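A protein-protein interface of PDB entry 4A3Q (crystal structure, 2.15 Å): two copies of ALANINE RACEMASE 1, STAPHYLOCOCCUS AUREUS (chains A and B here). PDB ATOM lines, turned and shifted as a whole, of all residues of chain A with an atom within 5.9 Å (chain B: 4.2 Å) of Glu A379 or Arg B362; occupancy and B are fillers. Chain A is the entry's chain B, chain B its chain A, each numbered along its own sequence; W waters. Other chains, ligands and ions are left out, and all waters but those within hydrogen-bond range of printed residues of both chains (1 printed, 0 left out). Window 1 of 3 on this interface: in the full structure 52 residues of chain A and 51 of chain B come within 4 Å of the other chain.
The guanidinium group (NH2) of Arg B362 lies within salt-bridge range of the side-chain carboxylate (OE2) of Glu A72. The side-chain carboxylate (OE1) of Glu A379 lies within salt-bridge range of the guanidinium group (NE) of Arg B362, 2.7 Å away. NE of Arg A362 lies within salt-bridge range of OE1 of Glu B379 (3.3 Å).
The side-chain hydroxyl of Ser B361 lies within hydrogen-bond range of the backbone NH of Arg B363 (3.0 Å). N of Ser A47 lies within hydrogen-bond range of OD1 of Asn A41 (3.0 Å).
Among the printed residues, merely in contact across the chains: Glu A379 with Glu B379 (3.2 Å), Glu A72 with Leu B380 (3.2 Å), Asn A41 with Arg B362 (3.4 Å) and Ala A40 with Arg B363 (3.8 Å).
Glu A379 touches just these residues of chain B: Arg B362 and Glu B379. Arg B362 touches just these residues of chain A: Asn A41, Glu A72 and Glu A379. Printed residues of chain B within 4 Å of Glu A72: Arg B362 and Leu B380. Of the printed residues of chain A, Arg B363 touches Ala A40 (3.8 Å). Printed residues of chain B within 4 Å of Asn A41: Arg B362 (3.4 Å). The nearest residue of chain A that does not touch Arg B362 is Arg A362 (4.5 Å). The nearest printed residue of chain B that does not touch Asn A41 is Arg B363 (5.6 Å).
Among the printed residues, Asp or Glu carboxylates within 4 Å of a Lys or Arg side-chain nitrogen of the other chain: Glu A72 with Arg B362, Arg A362 with Glu B379 and Glu A379 with Arg B362.
Arg A362 touches Glu B379, and with the chains exchanged Glu A379 touches Arg B362. Glu A379 touches its own counterpart, Glu B379. 4 positions are printed for both chains. Of the 7 pairs that touch across the chains among the printed residues, 3 have their exchanged pair printed and touching as well.
Water W1 lies within hydrogen-bond range of the side-chain carboxylate of Glu A72 (2.6 Å), the guanidinium group of Arg B362 (2.8 Å), the side-chain amide oxygen of Asn A41 (3.1 Å) and the side-chain hydroxyl of Ser A47 (3.5 Å).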
ATOM      1  N   ASP A   3      11.755  14.956 -28.410  1.00  0.00           N
ATOM      2  CA  ASP A   3      11.567  16.305 -27.825  1.00  0.00           C
ATOM      3  C   ASP A   3      11.178  17.388 -28.849  1.00  0.00           C
ATOM      4  O   ASP A   3      11.578  17.344 -30.016  1.00  0.00           O
ATOM      5  CB  ASP A   3      12.839  16.784 -27.111  1.00  0.00           C
ATOM      6  CG  ASP A   3      13.206  15.940 -25.922  1.00  0.00           C
ATOM      7  OD1 ASP A   3      12.342  15.199 -25.430  1.00  0.00           O
ATOM      8  OD2 ASP A   3      14.365  16.025 -25.467  1.00  0.00           O
ATOM      9  N   ALA A  40      32.484  12.372 -22.335  1.00  0.00           N
ATOM     10  CA  ALA A  40      32.123  13.779 -22.599  1.00  0.00           C
ATOM     11  C   ALA A  40      30.890  13.881 -23.452  1.00  0.00           C
ATOM     12  O   ALA A  40      30.869  14.641 -24.421  1.00  0.00           O
ATOM     13  CB  ALA A  40      33.280  14.537 -23.235  1.00  0.00           C
ATOM     14  N   ASN A  41      29.854  13.114 -23.099  1.00  0.00           N
ATOM     15  CA  ASN A  41      28.586  13.141 -23.861  1.00  0.00           C
ATOM     16  C   ASN A  41      28.803  12.817 -25.342  1.00  0.00           C
ATOM     17  O   ASN A  41      28.263  13.500 -26.239  1.00  0.00           O
ATOM     18  CB  ASN A  41      27.937  14.527 -23.709  1.00  0.00           C
ATOM     19  CG  ASN A  41      26.490  14.535 -24.066  1.00  0.00           C
ATOM     20  OD1 ASN A  41      25.790  13.555 -23.841  1.00  0.00           O
ATOM     21  ND2 ASN A  41      26.007  15.665 -24.598  1.00  0.00           N
ATOM     22  N   SER A  47      25.773  11.167 -25.623  1.00  0.00           N
ATOM     23  CA  SER A  47      26.261   9.804 -25.387  1.00  0.00           C
ATOM     24  C   SER A  47      25.151   8.765 -25.328  1.00  0.00           C
ATOM     25  O   SER A  47      25.342   7.645 -25.810  1.00  0.00           O
ATOM     26  CB  SER A  47      27.123   9.706 -24.122  1.00  0.00           C
ATOM     27  OG  SER A  47      26.330  10.017 -22.992  1.00  0.00           O
ATOM     28  N   GLU A  72      24.629   7.341 -16.217  1.00  0.00           N
ATOM     29  CA  GLU A  72      23.704   7.931 -17.182  1.00  0.00           C
ATOM     30  C   GLU A  72      23.379   6.884 -18.294  1.00  0.00           C
ATOM     31  O   GLU A  72      22.234   6.694 -18.661  1.00  0.00           O
ATOM     32  CB  GLU A  72      24.311   9.203 -17.781  1.00  0.00           C
ATOM     33  CG  GLU A  72      23.399   9.916 -18.782  1.00  0.00           C
ATOM     34  CD  GLU A  72      24.065  11.098 -19.502  1.00  0.00           C
ATOM     35  OE1 GLU A  72      25.302  11.199 -19.541  1.00  0.00           O
ATOM     36  OE2 GLU A  72      23.325  11.903 -20.083  1.00  0.00           O
ATOM     37  N   ARG A 362      24.453  22.661 -23.979  1.00  0.00           N
ATOM     38  CA  ARG A 362      23.198  21.936 -23.696  1.00  0.00           C
ATOM     39  C   ARG A 362      21.975  22.571 -24.339  1.00  0.00           C
ATOM     40  O   ARG A 362      20.953  21.907 -24.581  1.00  0.00           O
ATOM     41  CB  ARG A 362      22.974  21.848 -22.163  1.00  0.00           C
ATOM     42  CG  ARG A 362      22.908  23.228 -21.401  1.00  0.00           C
ATOM     43  CD  ARG A 362      22.839  23.099 -19.865  1.00  0.00           C
ATOM     44  NE  ARG A 362      21.591  22.528 -19.320  1.00  0.00           N
ATOM     45  CZ  ARG A 362      20.441  23.205 -19.194  1.00  0.00           C
ATOM     46  NH1 ARG A 362      20.378  24.469 -19.598  1.00  0.00           N
ATOM     47  NH2 ARG A 362      19.343  22.631 -18.657  1.00  0.00           N
ATOM     48  N   LEU A 364      21.499  23.665 -27.266  1.00  0.00           N
ATOM     49  CA  LEU A 364      21.250  23.269 -28.666  1.00  0.00           C
ATOM     50  C   LEU A 364      20.498  21.938 -28.736  1.00  0.00           C
ATOM     51  O   LEU A 364      20.992  20.910 -28.253  1.00  0.00           O
ATOM     52  CB  LEU A 364      22.577  23.163 -29.450  1.00  0.00           C
ATOM     53  CG  LEU A 364      23.320  24.491 -29.690  1.00  0.00           C
ATOM     54  CD1 LEU A 364      24.777  24.253 -30.048  1.00  0.00           C
ATOM     55  CD2 LEU A 364      22.626  25.319 -30.785  1.00  0.00           C
ATOM     56  N   PRO A 365      19.297  21.937 -29.331  1.00  0.00           N
ATOM     57  CA  PRO A 365      18.723  20.604 -29.573  1.00  0.00           C
ATOM     58  C   PRO A 365      19.675  19.802 -30.462  1.00  0.00           C
ATOM     59  O   PRO A 365      20.374  20.398 -31.320  1.00  0.00           O
ATOM     60  CB  PRO A 365      17.412  20.908 -30.320  1.00  0.00           C
ATOM     61  CG  PRO A 365      17.126  22.401 -29.987  1.00  0.00           C
ATOM     62  CD  PRO A 365      18.491  23.014 -29.934  1.00  0.00           C
ATOM     63  N   THR A 377      16.659  15.479 -29.230  1.00  0.00           N
ATOM     64  CA  THR A 377      16.910  15.642 -27.811  1.00  0.00           C
ATOM     65  C   THR A 377      17.004  17.144 -27.531  1.00  0.00           C
ATOM     66  O   THR A 377      17.714  17.861 -28.233  1.00  0.00           O
ATOM     67  CB  THR A 377      18.219  14.939 -27.382  1.00  0.00           C
ATOM     68  OG1 THR A 377      17.991  13.527 -27.338  1.00  0.00           O
ATOM     69  CG2 THR A 377      18.618  15.351 -25.984  1.00  0.00           C
ATOM     70  N   ASN A 378      16.290  17.589 -26.502  1.00  0.00           N
ATOM     71  CA  ASN A 378      16.295  18.973 -26.058  1.00  0.00           C
ATOM     72  C   ASN A 378      16.328  19.012 -24.535  1.00  0.00           C
ATOM     73  O   ASN A 378      15.287  18.900 -23.861  1.00  0.00           O
ATOM     74  CB  ASN A 378      15.079  19.705 -26.621  1.00  0.00           C
ATOM     75  CG  ASN A 378      15.040  21.182 -26.235  1.00  0.00           C
ATOM     76  OD1 ASN A 378      15.927  21.692 -25.547  1.00  0.00           O
ATOM     77  ND2 ASN A 378      13.986  21.874 -26.673  1.00  0.00           N
ATOM     78  N   GLU A 379      17.534  19.200 -24.006  1.00  0.00           N
ATOM     79  CA  GLU A 379      17.814  19.023 -22.581  1.00  0.00           C
ATOM     80  C   GLU A 379      17.030  19.950 -21.681  1.00  0.00           C
ATOM     81  O   GLU A 379      16.801  19.626 -20.516  1.00  0.00           O
ATOM     82  CB  GLU A 379      19.317  19.148 -22.291  1.00  0.00           C
ATOM     83  CG  GLU A 379      19.753  18.346 -21.048  1.00  0.00           C
ATOM     84  CD  GLU A 379      21.032  17.525 -21.250  1.00  0.00           C
ATOM     85  OE1 GLU A 379      22.124  18.123 -21.375  1.00  0.00           O
ATOM     86  OE2 GLU A 379      20.953  16.272 -21.252  1.00  0.00           O
ATOM     87  N   LEU A 380      16.610  21.091 -22.222  1.00  0.00           N
ATOM     88  CA  LEU A 380      15.873  22.087 -21.449  1.00  0.00           C
ATOM     89  C   LEU A 380      14.491  21.629 -21.100  1.00  0.00           C
ATOM     90  O   LEU A 380      13.960  22.057 -20.101  1.00  0.00           O
ATOM     91  CB  LEU A 380      15.799  23.435 -22.190  1.00  0.00           C
ATOM     92  CG  LEU A 380      16.997  24.366 -21.962  1.00  0.00           C
ATOM     93  CD1 LEU A 380      18.343  23.700 -22.317  1.00  0.00           C
ATOM     94  CD2 LEU A 380      16.806  25.723 -22.699  1.00  0.00           C
ATOM     95  N   LEU A 381      13.907  20.758 -21.922  1.00  0.00           N
ATOM     96  CA  LEU A 381      12.539  20.289 -21.679  1.00  0.00           C
ATOM     97  C   LEU A 381      12.482  18.873 -21.092  1.00  0.00           C
ATOM     98  O   LEU A 381      11.438  18.233 -21.092  1.00  0.00           O
ATOM     99  CB  LEU A 381      11.708  20.364 -22.969  1.00  0.00           C
ATOM    100  CG  LEU A 381      11.709  21.677 -23.764  1.00  0.00           C
ATOM    101  CD1 LEU A 381      10.867  21.504 -25.017  1.00  0.00           C
ATOM    102  CD2 LEU A 381      11.208  22.861 -22.938  1.00  0.00           C
ATOM    103  N   LYS A 382      13.605  18.374 -20.591  1.00  0.00           N
ATOM    104  CA  LYS A 382      13.609  17.050 -19.989  1.00  0.00           C
ATOM    105  C   LYS A 382      13.217  17.178 -18.530  1.00  0.00           C
ATOM    106  O   LYS A 382      12.215  16.599 -18.120  1.00  0.00           O
ATOM    107  CB  LYS A 382      14.973  16.382 -20.138  1.00  0.00           C
ATOM    108  CG  LYS A 382      15.250  15.915 -21.567  1.00  0.00           C
ATOM    109  CD  LYS A 382      16.697  15.388 -21.741  1.00  0.00           C
ATOM    110  CE  LYS A 382      16.810  14.217 -22.762  1.00  0.00           C
ATOM    111  NZ  LYS A 382      15.799  14.222 -23.903  1.00  0.00           N
ATOM    112  N   LEU B 360      31.095  26.750 -18.701  1.00  0.00           N
ATOM    113  CA  LEU B 360      31.055  25.679 -17.687  1.00  0.00           C
ATOM    114  C   LEU B 360      29.955  24.649 -18.005  1.00  0.00           C
ATOM    115  O   LEU B 360      28.748  24.953 -18.003  1.00  0.00           O
ATOM    116  CB  LEU B 360      30.929  26.248 -16.271  1.00  0.00           C
ATOM    117  CG  LEU B 360      32.013  27.285 -15.935  1.00  0.00           C
ATOM    118  CD1 LEU B 360      31.738  27.944 -14.576  1.00  0.00           C
ATOM    119  CD2 LEU B 360      33.417  26.662 -15.957  1.00  0.00           C
ATOM    120  N   SER B 361      30.407  23.443 -18.328  1.00  0.00           N
ATOM    121  CA  SER B 361      29.552  22.478 -18.978  1.00  0.00           C
ATOM    122  C   SER B 361      28.574  21.800 -18.035  1.00  0.00           C
ATOM    123  O   SER B 361      28.733  21.831 -16.799  1.00  0.00           O
ATOM    124  CB  SER B 361      30.396  21.440 -19.748  1.00  0.00           C
ATOM    125  OG  SER B 361      30.498  20.208 -19.046  1.00  0.00           O
ATOM    126  N   ARG B 362      27.582  21.168 -18.650  1.00  0.00           N
ATOM    127  CA  ARG B 362      26.566  20.339 -17.973  1.00  0.00           C
ATOM    128  C   ARG B 362      27.193  19.254 -17.109  1.00  0.00           C
ATOM    129  O   ARG B 362      26.584  18.797 -16.163  1.00  0.00           O
ATOM    130  CB  ARG B 362      25.654  19.662 -19.037  1.00  0.00           C
ATOM    131  CG  ARG B 362      26.406  18.705 -20.067  1.00  0.00           C
ATOM    132  CD  ARG B 362      25.537  18.182 -21.269  1.00  0.00           C
ATOM    133  NE  ARG B 362      24.545  17.151 -20.900  1.00  0.00           N
ATOM    134  CZ  ARG B 362      24.838  15.862 -20.684  1.00  0.00           C
ATOM    135  NH1 ARG B 362      26.105  15.461 -20.791  1.00  0.00           N
ATOM    136  NH2 ARG B 362      23.871  14.963 -20.368  1.00  0.00           N
ATOM    137  N   ARG B 363      28.414  18.843 -17.440  1.00  0.00           N
ATOM    138  CA  ARG B 363      29.034  17.733 -16.723  1.00  0.00           C
ATOM    139  C   ARG B 363      29.402  18.062 -15.269  1.00  0.00           C
ATOM    140  O   ARG B 363      29.538  17.151 -14.437  1.00  0.00           O
ATOM    141  CB  ARG B 363      30.246  17.203 -17.483  1.00  0.00           C
ATOM    142  CG  ARG B 363      30.805  15.923 -16.904  1.00  0.00           C
ATOM    143  CD  ARG B 363      31.689  15.218 -17.883  1.00  0.00           C
ATOM    144  NE  ARG B 363      33.001  15.865 -17.999  1.00  0.00           N
ATOM    145  CZ  ARG B 363      34.013  15.309 -18.651  1.00  0.00           C
ATOM    146  NH1 ARG B 363      33.820  14.132 -19.238  1.00  0.00           N
ATOM    147  NH2 ARG B 363      35.200  15.913 -18.731  1.00  0.00           N
ATOM    148  N   LEU B 364      29.575  19.344 -14.968  1.00  0.00           N
ATOM    149  CA  LEU B 364      29.915  19.757 -13.603  1.00  0.00           C
ATOM    150  C   LEU B 364      28.663  19.834 -12.761  1.00  0.00           C
ATOM    151  O   LEU B 364      27.755  20.564 -13.118  1.00  0.00           O
ATOM    152  CB  LEU B 364      30.578  21.137 -13.617  1.00  0.00           C
ATOM    153  CG  LEU B 364      31.967  21.202 -14.233  1.00  0.00           C
ATOM    154  CD1 LEU B 364      32.275  22.647 -14.614  1.00  0.00           C
ATOM    155  CD2 LEU B 364      32.988  20.620 -13.227  1.00  0.00           C
ATOM    156  N   GLU B 379      23.167  17.085 -13.838  1.00  0.00           N
ATOM    157  CA  GLU B 379      22.458  16.892 -15.083  1.00  0.00           C
ATOM    158  C   GLU B 379      22.550  15.453 -15.647  1.00  0.00           C
ATOM    159  O   GLU B 379      21.572  14.928 -16.215  1.00  0.00           O
ATOM    160  CB  GLU B 379      23.043  17.867 -16.114  1.00  0.00           C
ATOM    161  CG  GLU B 379      22.440  17.791 -17.484  1.00  0.00           C
ATOM    162  CD  GLU B 379      21.150  18.605 -17.588  1.00  0.00           C
ATOM    163  OE1 GLU B 379      21.187  19.846 -17.375  1.00  0.00           O
ATOM    164  OE2 GLU B 379      20.112  17.992 -17.909  1.00  0.00           O
ATOM    165  N   LEU B 380      23.720  14.832 -15.517  1.00  0.00           N
ATOM    166  CA  LEU B 380      23.915  13.474 -16.059  1.00  0.00           C
ATOM    167  C   LEU B 380      23.002  12.427 -15.413  1.00  0.00           C
ATOM    168  O   LEU B 380      22.698  11.433 -16.046  1.00  0.00           O
ATOM    169  CB  LEU B 380      25.365  13.014 -15.945  1.00  0.00           C
ATOM    170  CG  LEU B 380      26.276  13.417 -17.117  1.00  0.00           C
ATOM    171  CD1 LEU B 380      26.329  14.958 -17.299  1.00  0.00           C
ATOM    172  CD2 LEU B 380      27.685  12.841 -16.890  1.00  0.00           C
HETATM  173  O   HOH W   1      26.812  12.793 -20.978  1.00  0.00           O
